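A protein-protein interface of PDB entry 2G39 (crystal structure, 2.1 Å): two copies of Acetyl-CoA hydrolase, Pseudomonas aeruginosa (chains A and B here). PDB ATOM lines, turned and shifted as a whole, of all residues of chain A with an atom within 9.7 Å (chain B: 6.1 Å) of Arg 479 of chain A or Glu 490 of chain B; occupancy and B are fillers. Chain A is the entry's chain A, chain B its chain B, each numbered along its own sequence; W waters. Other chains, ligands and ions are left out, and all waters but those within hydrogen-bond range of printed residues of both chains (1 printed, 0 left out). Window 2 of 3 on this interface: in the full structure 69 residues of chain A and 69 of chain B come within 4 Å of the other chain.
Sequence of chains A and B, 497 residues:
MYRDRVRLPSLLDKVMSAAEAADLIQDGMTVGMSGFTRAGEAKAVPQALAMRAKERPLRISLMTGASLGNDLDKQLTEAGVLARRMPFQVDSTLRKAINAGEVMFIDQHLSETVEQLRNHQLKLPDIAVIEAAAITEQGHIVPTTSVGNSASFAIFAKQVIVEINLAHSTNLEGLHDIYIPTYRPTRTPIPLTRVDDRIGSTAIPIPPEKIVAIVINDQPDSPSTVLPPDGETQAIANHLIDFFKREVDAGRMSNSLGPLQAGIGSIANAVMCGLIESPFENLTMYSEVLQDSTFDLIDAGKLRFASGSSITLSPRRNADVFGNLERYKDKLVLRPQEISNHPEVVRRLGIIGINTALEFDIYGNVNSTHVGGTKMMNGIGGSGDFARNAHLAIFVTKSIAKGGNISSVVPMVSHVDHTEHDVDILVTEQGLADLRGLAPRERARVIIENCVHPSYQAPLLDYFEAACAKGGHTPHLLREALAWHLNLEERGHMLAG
3 positions are printed for both chains.
Water W1 bridges the guanidinium group of Arg 479 of chain A (2.9 Å) and the guanidinium group of Arg 491 of chain B (3.3 Å).
The side-chain carboxylate (OE2) of Glu 490 of chain B lies within salt-bridge range of the guanidinium group (NH2) of Arg 479 of chain A, at 3.8 Å.
Of the printed residues of chain B, Leu 478 of chain A touches His 485, Leu 486 and Glu 489.
Arg 479 of chain A touches just these residues of chain B: Leu 486 and Glu 490.
Asn 487 of chain A touches none of the printed residues of chain B.
Of the printed residues of chain A, His 485 of chain B touches Leu 478 (3.8 Å).
Of the printed residues of chain A, Leu 486 of chain B touches Leu 478 (3.8 Å) and Arg 479 (3.6 Å).
Printed residues of chain A within 4 Å of Glu 489 of chain B: Leu 478.
No residue of chain A comes within 4 Å of Arg 491 of chain B.
The nearest residue of chain B that does not touch Arg 479 of chain A is Arg 491 of chain B (4.6 Å).
The nearest printed residue of chain A that does not touch His 485 of chain B is Arg 479 of chain A (8.1 Å).
Of the 8 printed residues of chain B, 4 touch a printed residue of chain A.
Printed residues of chain B that touch a printed residue of chain A: His 485, Leu 486, Glu 489 and Glu 490.
Among the printed residues, 5 pairs touch across the chains.
Among the printed residues, Asp or Glu carboxylates within 4 Å of a Lys or Arg side-chain nitrogen of the other chain: Arg 479 of chain A with Glu 490 of chain B (3.8 Å).
His 485 of chain B touches Leu 478 of chain A (C to CD1, 3.8 Å).
Leu 486 of chain B touches Leu 478 of chain A.
Leu 478 of chain A touches Glu 489 of chain B.
Leu 486 of chain B touches Arg 479 of chain A (CD2 to CG, 3.6 Å).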
ATOM      1  N   PRO A 411     -22.121   6.528 -14.840  1.00  0.00           N
ATOM      2  CA  PRO A 411     -21.566   6.265 -16.191  1.00  0.00           C
ATOM      3  C   PRO A 411     -20.109   6.776 -16.348  1.00  0.00           C
ATOM      4  O   PRO A 411     -19.256   6.091 -16.912  1.00  0.00           O
ATOM      5  CB  PRO A 411     -22.526   7.030 -17.096  1.00  0.00           C
ATOM      6  CG  PRO A 411     -23.826   7.071 -16.271  1.00  0.00           C
ATOM      7  CD  PRO A 411     -23.329   7.358 -14.904  1.00  0.00           C
ATOM      8  N   MET A 412     -19.855   7.968 -15.811  1.00  0.00           N
ATOM      9  CA  MET A 412     -18.560   8.594 -15.849  1.00  0.00           C
ATOM     10  C   MET A 412     -18.425   9.415 -14.557  1.00  0.00           C
ATOM     11  O   MET A 412     -19.328  10.161 -14.209  1.00  0.00           O
ATOM     12  CB  MET A 412     -18.437   9.515 -17.073  1.00  0.00           C
ATOM     13  CG  MET A 412     -17.129  10.306 -17.077  1.00  0.00           C
ATOM     14  SD  MET A 412     -17.032  11.698 -18.490  1.00  0.00           S
ATOM     15  CE  MET A 412     -16.542  10.488 -20.084  1.00  0.00           C
ATOM     16  N   TYR A 463     -27.180   2.825 -20.547  1.00  0.00           N
ATOM     17  CA  TYR A 463     -26.132   3.779 -20.929  1.00  0.00           C
ATOM     18  C   TYR A 463     -24.985   3.033 -21.619  1.00  0.00           C
ATOM     19  O   TYR A 463     -24.552   3.421 -22.702  1.00  0.00           O
ATOM     20  CB  TYR A 463     -25.596   4.554 -19.704  1.00  0.00           C
ATOM     21  CG  TYR A 463     -24.378   5.408 -20.044  1.00  0.00           C
ATOM     22  CD1 TYR A 463     -24.530   6.733 -20.468  1.00  0.00           C
ATOM     23  CD2 TYR A 463     -23.090   4.879 -20.002  1.00  0.00           C
ATOM     24  CE1 TYR A 463     -23.424   7.499 -20.830  1.00  0.00           C
ATOM     25  CE2 TYR A 463     -21.974   5.660 -20.342  1.00  0.00           C
ATOM     26  CZ  TYR A 463     -22.165   6.956 -20.751  1.00  0.00           C
ATOM     27  OH  TYR A 463     -21.114   7.721 -21.078  1.00  0.00           O
ATOM     28  N   ALA A 467     -23.902   3.446 -25.479  1.00  0.00           N
ATOM     29  CA  ALA A 467     -22.513   3.903 -25.691  1.00  0.00           C
ATOM     30  C   ALA A 467     -21.727   2.953 -26.604  1.00  0.00           C
ATOM     31  O   ALA A 467     -21.063   3.403 -27.545  1.00  0.00           O
ATOM     32  CB  ALA A 467     -21.786   4.070 -24.343  1.00  0.00           C
ATOM     33  N   LYS A 470     -22.107   3.246 -30.283  1.00  0.00           N
ATOM     34  CA  LYS A 470     -21.307   4.329 -30.894  1.00  0.00           C
ATOM     35  C   LYS A 470     -19.800   4.019 -30.959  1.00  0.00           C
ATOM     36  O   LYS A 470     -19.000   4.867 -31.405  1.00  0.00           O
ATOM     37  CB  LYS A 470     -21.511   5.643 -30.139  1.00  0.00           C
ATOM     38  CG  LYS A 470     -22.800   6.358 -30.448  1.00  0.00           C
ATOM     39  CD  LYS A 470     -22.896   7.598 -29.554  1.00  0.00           C
ATOM     40  CE  LYS A 470     -24.009   8.590 -29.972  1.00  0.00           C
ATOM     41  NZ  LYS A 470     -25.030   8.032 -30.900  1.00  0.00           N
ATOM     42  N   HIS A 476     -18.715   5.842 -24.527  1.00  0.00           N
ATOM     43  CA  HIS A 476     -19.484   6.852 -23.799  1.00  0.00           C
ATOM     44  C   HIS A 476     -20.487   7.536 -24.717  1.00  0.00           C
ATOM     45  O   HIS A 476     -20.324   7.570 -25.941  1.00  0.00           O
ATOM     46  CB  HIS A 476     -18.573   7.924 -23.190  1.00  0.00           C
ATOM     47  CG  HIS A 476     -17.930   7.514 -21.902  1.00  0.00           C
ATOM     48  ND1 HIS A 476     -18.651   7.290 -20.749  1.00  0.00           N
ATOM     49  CD2 HIS A 476     -16.627   7.293 -21.584  1.00  0.00           C
ATOM     50  CE1 HIS A 476     -17.821   6.933 -19.779  1.00  0.00           C
ATOM     51  NE2 HIS A 476     -16.589   6.952 -20.252  1.00  0.00           N
ATOM     52  N   LEU A 477     -21.514   8.098 -24.106  1.00  0.00           N
ATOM     53  CA  LEU A 477     -22.408   9.031 -24.779  1.00  0.00           C
ATOM     54  C   LEU A 477     -22.037  10.400 -24.224  1.00  0.00           C
ATOM     55  O   LEU A 477     -22.305  10.671 -23.048  1.00  0.00           O
ATOM     56  CB  LEU A 477     -23.862   8.678 -24.450  1.00  0.00           C
ATOM     57  CG  LEU A 477     -24.385   7.301 -24.910  1.00  0.00           C
ATOM     58  CD1 LEU A 477     -25.735   6.963 -24.270  1.00  0.00           C
ATOM     59  CD2 LEU A 477     -24.491   7.228 -26.409  1.00  0.00           C
ATOM     60  N   LEU A 478     -21.370  11.231 -25.028  1.00  0.00           N
ATOM     61  CA  LEU A 478     -20.980  12.580 -24.595  1.00  0.00           C
ATOM     62  C   LEU A 478     -22.173  13.433 -24.133  1.00  0.00           C
ATOM     63  O   LEU A 478     -22.006  14.316 -23.275  1.00  0.00           O
ATOM     64  CB  LEU A 478     -20.157  13.320 -25.672  1.00  0.00           C
ATOM     65  CG  LEU A 478     -18.793  12.675 -26.037  1.00  0.00           C
ATOM     66  CD1 LEU A 478     -18.125  13.256 -27.333  1.00  0.00           C
ATOM     67  CD2 LEU A 478     -17.815  12.703 -24.859  1.00  0.00           C
ATOM     68  N   ARG A 479     -23.364  13.148 -24.669  1.00  0.00           N
ATOM     69  CA  ARG A 479     -24.577  13.844 -24.257  1.00  0.00           C
ATOM     70  C   ARG A 479     -25.017  13.454 -22.875  1.00  0.00           C
ATOM     71  O   ARG A 479     -25.631  14.270 -22.187  1.00  0.00           O
ATOM     72  CB  ARG A 479     -25.735  13.569 -25.218  1.00  0.00           C
ATOM     73  CG  ARG A 479     -25.639  14.328 -26.472  1.00  0.00           C
ATOM     74  CD  ARG A 479     -26.989  14.446 -27.201  1.00  0.00           C
ATOM     75  NE  ARG A 479     -26.765  15.202 -28.431  1.00  0.00           N
ATOM     76  CZ  ARG A 479     -26.229  14.689 -29.533  1.00  0.00           C
ATOM     77  NH1 ARG A 479     -25.902  13.401 -29.573  1.00  0.00           N
ATOM     78  NH2 ARG A 479     -26.020  15.467 -30.597  1.00  0.00           N
ATOM     79  N   GLU A 480     -24.725  12.213 -22.476  1.00  0.00           N
ATOM     80  CA  GLU A 480     -25.289  11.649 -21.252  1.00  0.00           C
ATOM     81  C   GLU A 480     -24.285  11.342 -20.146  1.00  0.00           C
ATOM     82  O   GLU A 480     -24.698  11.039 -19.023  1.00  0.00           O
ATOM     83  CB  GLU A 480     -26.156  10.406 -21.562  1.00  0.00           C
ATOM     84  CG  GLU A 480     -27.283  10.633 -22.593  1.00  0.00           C
ATOM     85  CD  GLU A 480     -28.279  11.778 -22.239  1.00  0.00           C
ATOM     86  OE1 GLU A 480     -28.679  12.549 -23.171  1.00  0.00           O
ATOM     87  OE2 GLU A 480     -28.683  11.906 -21.050  1.00  0.00           O
ATOM     88  N   ALA A 481     -22.980  11.413 -20.446  1.00  0.00           N
ATOM     89  CA  ALA A 481     -21.935  10.951 -19.507  1.00  0.00           C
ATOM     90  C   ALA A 481     -22.071  11.609 -18.153  1.00  0.00           C
ATOM     91  O   ALA A 481     -21.897  10.934 -17.126  1.00  0.00           O
ATOM     92  CB  ALA A 481     -20.577  11.202 -20.050  1.00  0.00           C
ATOM     93  N   LEU A 482     -22.410  12.906 -18.159  1.00  0.00           N
ATOM     94  CA  LEU A 482     -22.526  13.673 -16.917  1.00  0.00           C
ATOM     95  C   LEU A 482     -23.967  14.026 -16.512  1.00  0.00           C
ATOM     96  O   LEU A 482     -24.161  14.798 -15.565  1.00  0.00           O
ATOM     97  CB  LEU A 482     -21.655  14.961 -16.977  1.00  0.00           C
ATOM     98  CG  LEU A 482     -20.130  14.832 -17.211  1.00  0.00           C
ATOM     99  CD1 LEU A 482     -19.496  16.233 -17.231  1.00  0.00           C
ATOM    100  CD2 LEU A 482     -19.468  13.971 -16.151  1.00  0.00           C
ATOM    101  N   ALA A 483     -24.949  13.459 -17.216  1.00  0.00           N
ATOM    102  CA  ALA A 483     -26.378  13.800 -17.047  1.00  0.00           C
ATOM    103  C   ALA A 483     -26.910  13.437 -15.653  1.00  0.00           C
ATOM    104  O   ALA A 483     -27.722  14.181 -15.112  1.00  0.00           O
ATOM    105  CB  ALA A 483     -27.253  13.102 -18.141  1.00  0.00           C
ATOM    106  N   TRP A 484     -26.458  12.310 -15.082  1.00  0.00           N
ATOM    107  CA  TRP A 484     -26.887  11.926 -13.719  1.00  0.00           C
ATOM    108  C   TRP A 484     -26.476  12.998 -12.707  1.00  0.00           C
ATOM    109  O   TRP A 484     -27.269  13.374 -11.849  1.00  0.00           O
ATOM    110  CB  TRP A 484     -26.366  10.549 -13.271  1.00  0.00           C
ATOM    111  CG  TRP A 484     -27.022   9.378 -13.963  1.00  0.00           C
ATOM    112  CD1 TRP A 484     -27.840   9.428 -15.053  1.00  0.00           C
ATOM    113  CD2 TRP A 484     -26.861   7.976 -13.654  1.00  0.00           C
ATOM    114  NE1 TRP A 484     -28.243   8.161 -15.413  1.00  0.00           N
ATOM    115  CE2 TRP A 484     -27.644   7.249 -14.588  1.00  0.00           C
ATOM    116  CE3 TRP A 484     -26.156   7.270 -12.674  1.00  0.00           C
ATOM    117  CZ2 TRP A 484     -27.719   5.851 -14.590  1.00  0.00           C
ATOM    118  CZ3 TRP A 484     -26.254   5.855 -12.657  1.00  0.00           C
ATOM    119  CH2 TRP A 484     -27.042   5.176 -13.604  1.00  0.00           C
ATOM    120  N   HIS A 485     -25.252  13.513 -12.860  1.00  0.00           N
ATOM    121  CA  HIS A 485     -24.745  14.581 -11.994  1.00  0.00           C
ATOM    122  C   HIS A 485     -25.541  15.875 -12.141  1.00  0.00           C
ATOM    123  O   HIS A 485     -25.829  16.549 -11.160  1.00  0.00           O
ATOM    124  CB  HIS A 485     -23.271  14.830 -12.291  1.00  0.00           C
ATOM    125  CG  HIS A 485     -22.409  13.626 -12.074  1.00  0.00           C
ATOM    126  ND1 HIS A 485     -22.069  13.173 -10.815  1.00  0.00           N
ATOM    127  CD2 HIS A 485     -21.788  12.805 -12.952  1.00  0.00           C
ATOM    128  CE1 HIS A 485     -21.310  12.101 -10.930  1.00  0.00           C
ATOM    129  NE2 HIS A 485     -21.127  11.857 -12.216  1.00  0.00           N
ATOM    130  N   LEU A 486     -25.876  16.212 -13.383  1.00  0.00           N
ATOM    131  CA  LEU A 486     -26.728  17.367 -13.668  1.00  0.00           C
ATOM    132  C   LEU A 486     -28.156  17.171 -13.136  1.00  0.00           C
ATOM    133  O   LEU A 486     -28.711  18.072 -12.509  1.00  0.00           O
ATOM    134  CB  LEU A 486     -26.705  17.651 -15.176  1.00  0.00           C
ATOM    135  CG  LEU A 486     -27.470  18.873 -15.672  1.00  0.00           C
ATOM    136  CD1 LEU A 486     -26.737  20.175 -15.278  1.00  0.00           C
ATOM    137  CD2 LEU A 486     -27.646  18.749 -17.206  1.00  0.00           C
ATOM    138  N   ASN A 487     -28.743  15.988 -13.356  1.00  0.00           N
ATOM    139  CA  ASN A 487     -30.078  15.641 -12.809  1.00  0.00           C
ATOM    140  C   ASN A 487     -30.089  15.794 -11.292  1.00  0.00           C
ATOM    141  O   ASN A 487     -31.005  16.387 -10.729  1.00  0.00           O
ATOM    142  CB  ASN A 487     -30.446  14.186 -13.143  1.00  0.00           C
ATOM    143  CG  ASN A 487     -30.712  13.951 -14.637  1.00  0.00           C
ATOM    144  OD1 ASN A 487     -30.897  14.904 -15.406  1.00  0.00           O
ATOM    145  ND2 ASN A 487     -30.748  12.659 -15.048  1.00  0.00           N
ATOM    146  N   HIS B 485     -16.280  18.471 -27.270  1.00  0.00           N
ATOM    147  CA  HIS B 485     -16.034  17.140 -27.848  1.00  0.00           C
ATOM    148  C   HIS B 485     -17.260  16.704 -28.646  1.00  0.00           C
ATOM    149  O   HIS B 485     -17.119  16.146 -29.713  1.00  0.00           O
ATOM    150  CB  HIS B 485     -15.677  16.111 -26.773  1.00  0.00           C
ATOM    151  CG  HIS B 485     -14.546  16.548 -25.892  1.00  0.00           C
ATOM    152  ND1 HIS B 485     -13.227  16.335 -26.221  1.00  0.00           N
ATOM    153  CD2 HIS B 485     -14.535  17.242 -24.726  1.00  0.00           C
ATOM    154  CE1 HIS B 485     -12.447  16.870 -25.295  1.00  0.00           C
ATOM    155  NE2 HIS B 485     -13.217  17.416 -24.369  1.00  0.00           N
ATOM    156  N   LEU B 486     -18.456  16.959 -28.112  1.00  0.00           N
ATOM    157  CA  LEU B 486     -19.709  16.672 -28.832  1.00  0.00           C
ATOM    158  C   LEU B 486     -19.821  17.496 -30.117  1.00  0.00           C
ATOM    159  O   LEU B 486     -20.174  16.958 -31.176  1.00  0.00           O
ATOM    160  CB  LEU B 486     -20.930  16.871 -27.910  1.00  0.00           C
ATOM    161  CG  LEU B 486     -22.287  16.490 -28.512  1.00  0.00           C
ATOM    162  CD1 LEU B 486     -22.365  14.976 -28.782  1.00  0.00           C
ATOM    163  CD2 LEU B 486     -23.461  16.984 -27.630  1.00  0.00           C
ATOM    164  N   ASN B 487     -19.504  18.792 -30.030  1.00  0.00           N
ATOM    165  CA  ASN B 487     -19.509  19.697 -31.206  1.00  0.00           C
ATOM    166  C   ASN B 487     -18.571  19.220 -32.308  1.00  0.00           C
ATOM    167  O   ASN B 487     -18.896  19.316 -33.505  1.00  0.00           O
ATOM    168  CB  ASN B 487     -19.061  21.097 -30.789  1.00  0.00           C
ATOM    169  CG  ASN B 487     -20.096  21.824 -29.949  1.00  0.00           C
ATOM    170  OD1 ASN B 487     -21.264  21.419 -29.871  1.00  0.00           O
ATOM    171  ND2 ASN B 487     -19.674  22.895 -29.319  1.00  0.00           N
ATOM    172  N   LEU B 488     -17.382  18.744 -31.895  1.00  0.00           N
ATOM    173  CA  LEU B 488     -16.381  18.264 -32.838  1.00  0.00           C
ATOM    174  C   LEU B 488     -16.946  17.068 -33.574  1.00  0.00           C
ATOM    175  O   LEU B 488     -16.904  17.003 -34.797  1.00  0.00           O
ATOM    176  CB  LEU B 488     -15.077  17.872 -32.128  1.00  0.00           C
ATOM    177  CG  LEU B 488     -13.979  17.274 -33.018  1.00  0.00           C
ATOM    178  CD1 LEU B 488     -13.632  18.264 -34.161  1.00  0.00           C
ATOM    179  CD2 LEU B 488     -12.711  16.892 -32.180  1.00  0.00           C
ATOM    180  N   GLU B 489     -17.482  16.136 -32.806  1.00  0.00           N
ATOM    181  CA  GLU B 489     -18.059  14.919 -33.328  1.00  0.00           C
ATOM    182  C   GLU B 489     -19.326  15.122 -34.184  1.00  0.00           C
ATOM    183  O   GLU B 489     -19.440  14.541 -35.264  1.00  0.00           O
ATOM    184  CB  GLU B 489     -18.390  14.029 -32.149  1.00  0.00           C
ATOM    185  CG  GLU B 489     -18.200  12.571 -32.413  1.00  0.00           C
ATOM    186  CD  GLU B 489     -18.114  11.817 -31.119  1.00  0.00           C
ATOM    187  OE1 GLU B 489     -16.959  11.659 -30.620  1.00  0.00           O
ATOM    188  OE2 GLU B 489     -19.206  11.448 -30.591  1.00  0.00           O
ATOM    189  N   GLU B 490     -20.273  15.934 -33.711  1.00  0.00           N
ATOM    190  CA  GLU B 490     -21.534  16.135 -34.446  1.00  0.00           C
ATOM    191  C   GLU B 490     -21.376  17.051 -35.646  1.00  0.00           C
ATOM    192  O   GLU B 490     -22.019  16.843 -36.693  1.00  0.00           O
ATOM    193  CB  GLU B 490     -22.616  16.722 -33.540  1.00  0.00           C
ATOM    194  CG  GLU B 490     -23.192  15.765 -32.500  1.00  0.00           C
ATOM    195  CD  GLU B 490     -23.476  14.394 -33.084  1.00  0.00           C
ATOM    196  OE1 GLU B 490     -22.668  13.472 -32.831  1.00  0.00           O
ATOM    197  OE2 GLU B 490     -24.486  14.236 -33.817  1.00  0.00           O
ATOM    198  N   ARG B 491     -20.540  18.081 -35.489  1.00  0.00           N
ATOM    199  CA  ARG B 491     -20.498  19.174 -36.460  1.00  0.00           C
ATOM    200  C   ARG B 491     -19.094  19.508 -36.999  1.00  0.00           C
ATOM    201  O   ARG B 491     -18.951  20.457 -37.773  1.00  0.00           O
ATOM    202  CB  ARG B 491     -21.234  20.412 -35.915  1.00  0.00           C
ATOM    203  CG  ARG B 491     -22.733  20.162 -35.653  1.00  0.00           C
ATOM    204  CD  ARG B 491     -23.364  21.147 -34.667  1.00  0.00           C
ATOM    205  NE  ARG B 491     -23.060  20.879 -33.253  1.00  0.00           N
ATOM    206  CZ  ARG B 491     -23.670  19.954 -32.498  1.00  0.00           C
ATOM    207  NH1 ARG B 491     -24.616  19.171 -33.019  1.00  0.00           N
ATOM    208  NH2 ARG B 491     -23.334  19.801 -31.217  1.00  0.00           N
ATOM    209  N   GLY B 492     -18.074  18.730 -36.612  1.00  0.00           N
ATOM    210  CA  GLY B 492     -16.747  18.841 -37.241  1.00  0.00           C
ATOM    211  C   GLY B 492     -15.889  19.996 -36.736  1.00  0.00           C
ATOM    212  O   GLY B 492     -14.736  20.156 -37.176  1.00  0.00           O
HETATM  213  O   HOH W   1     -26.077  18.301 -30.129  1.00  0.00           O
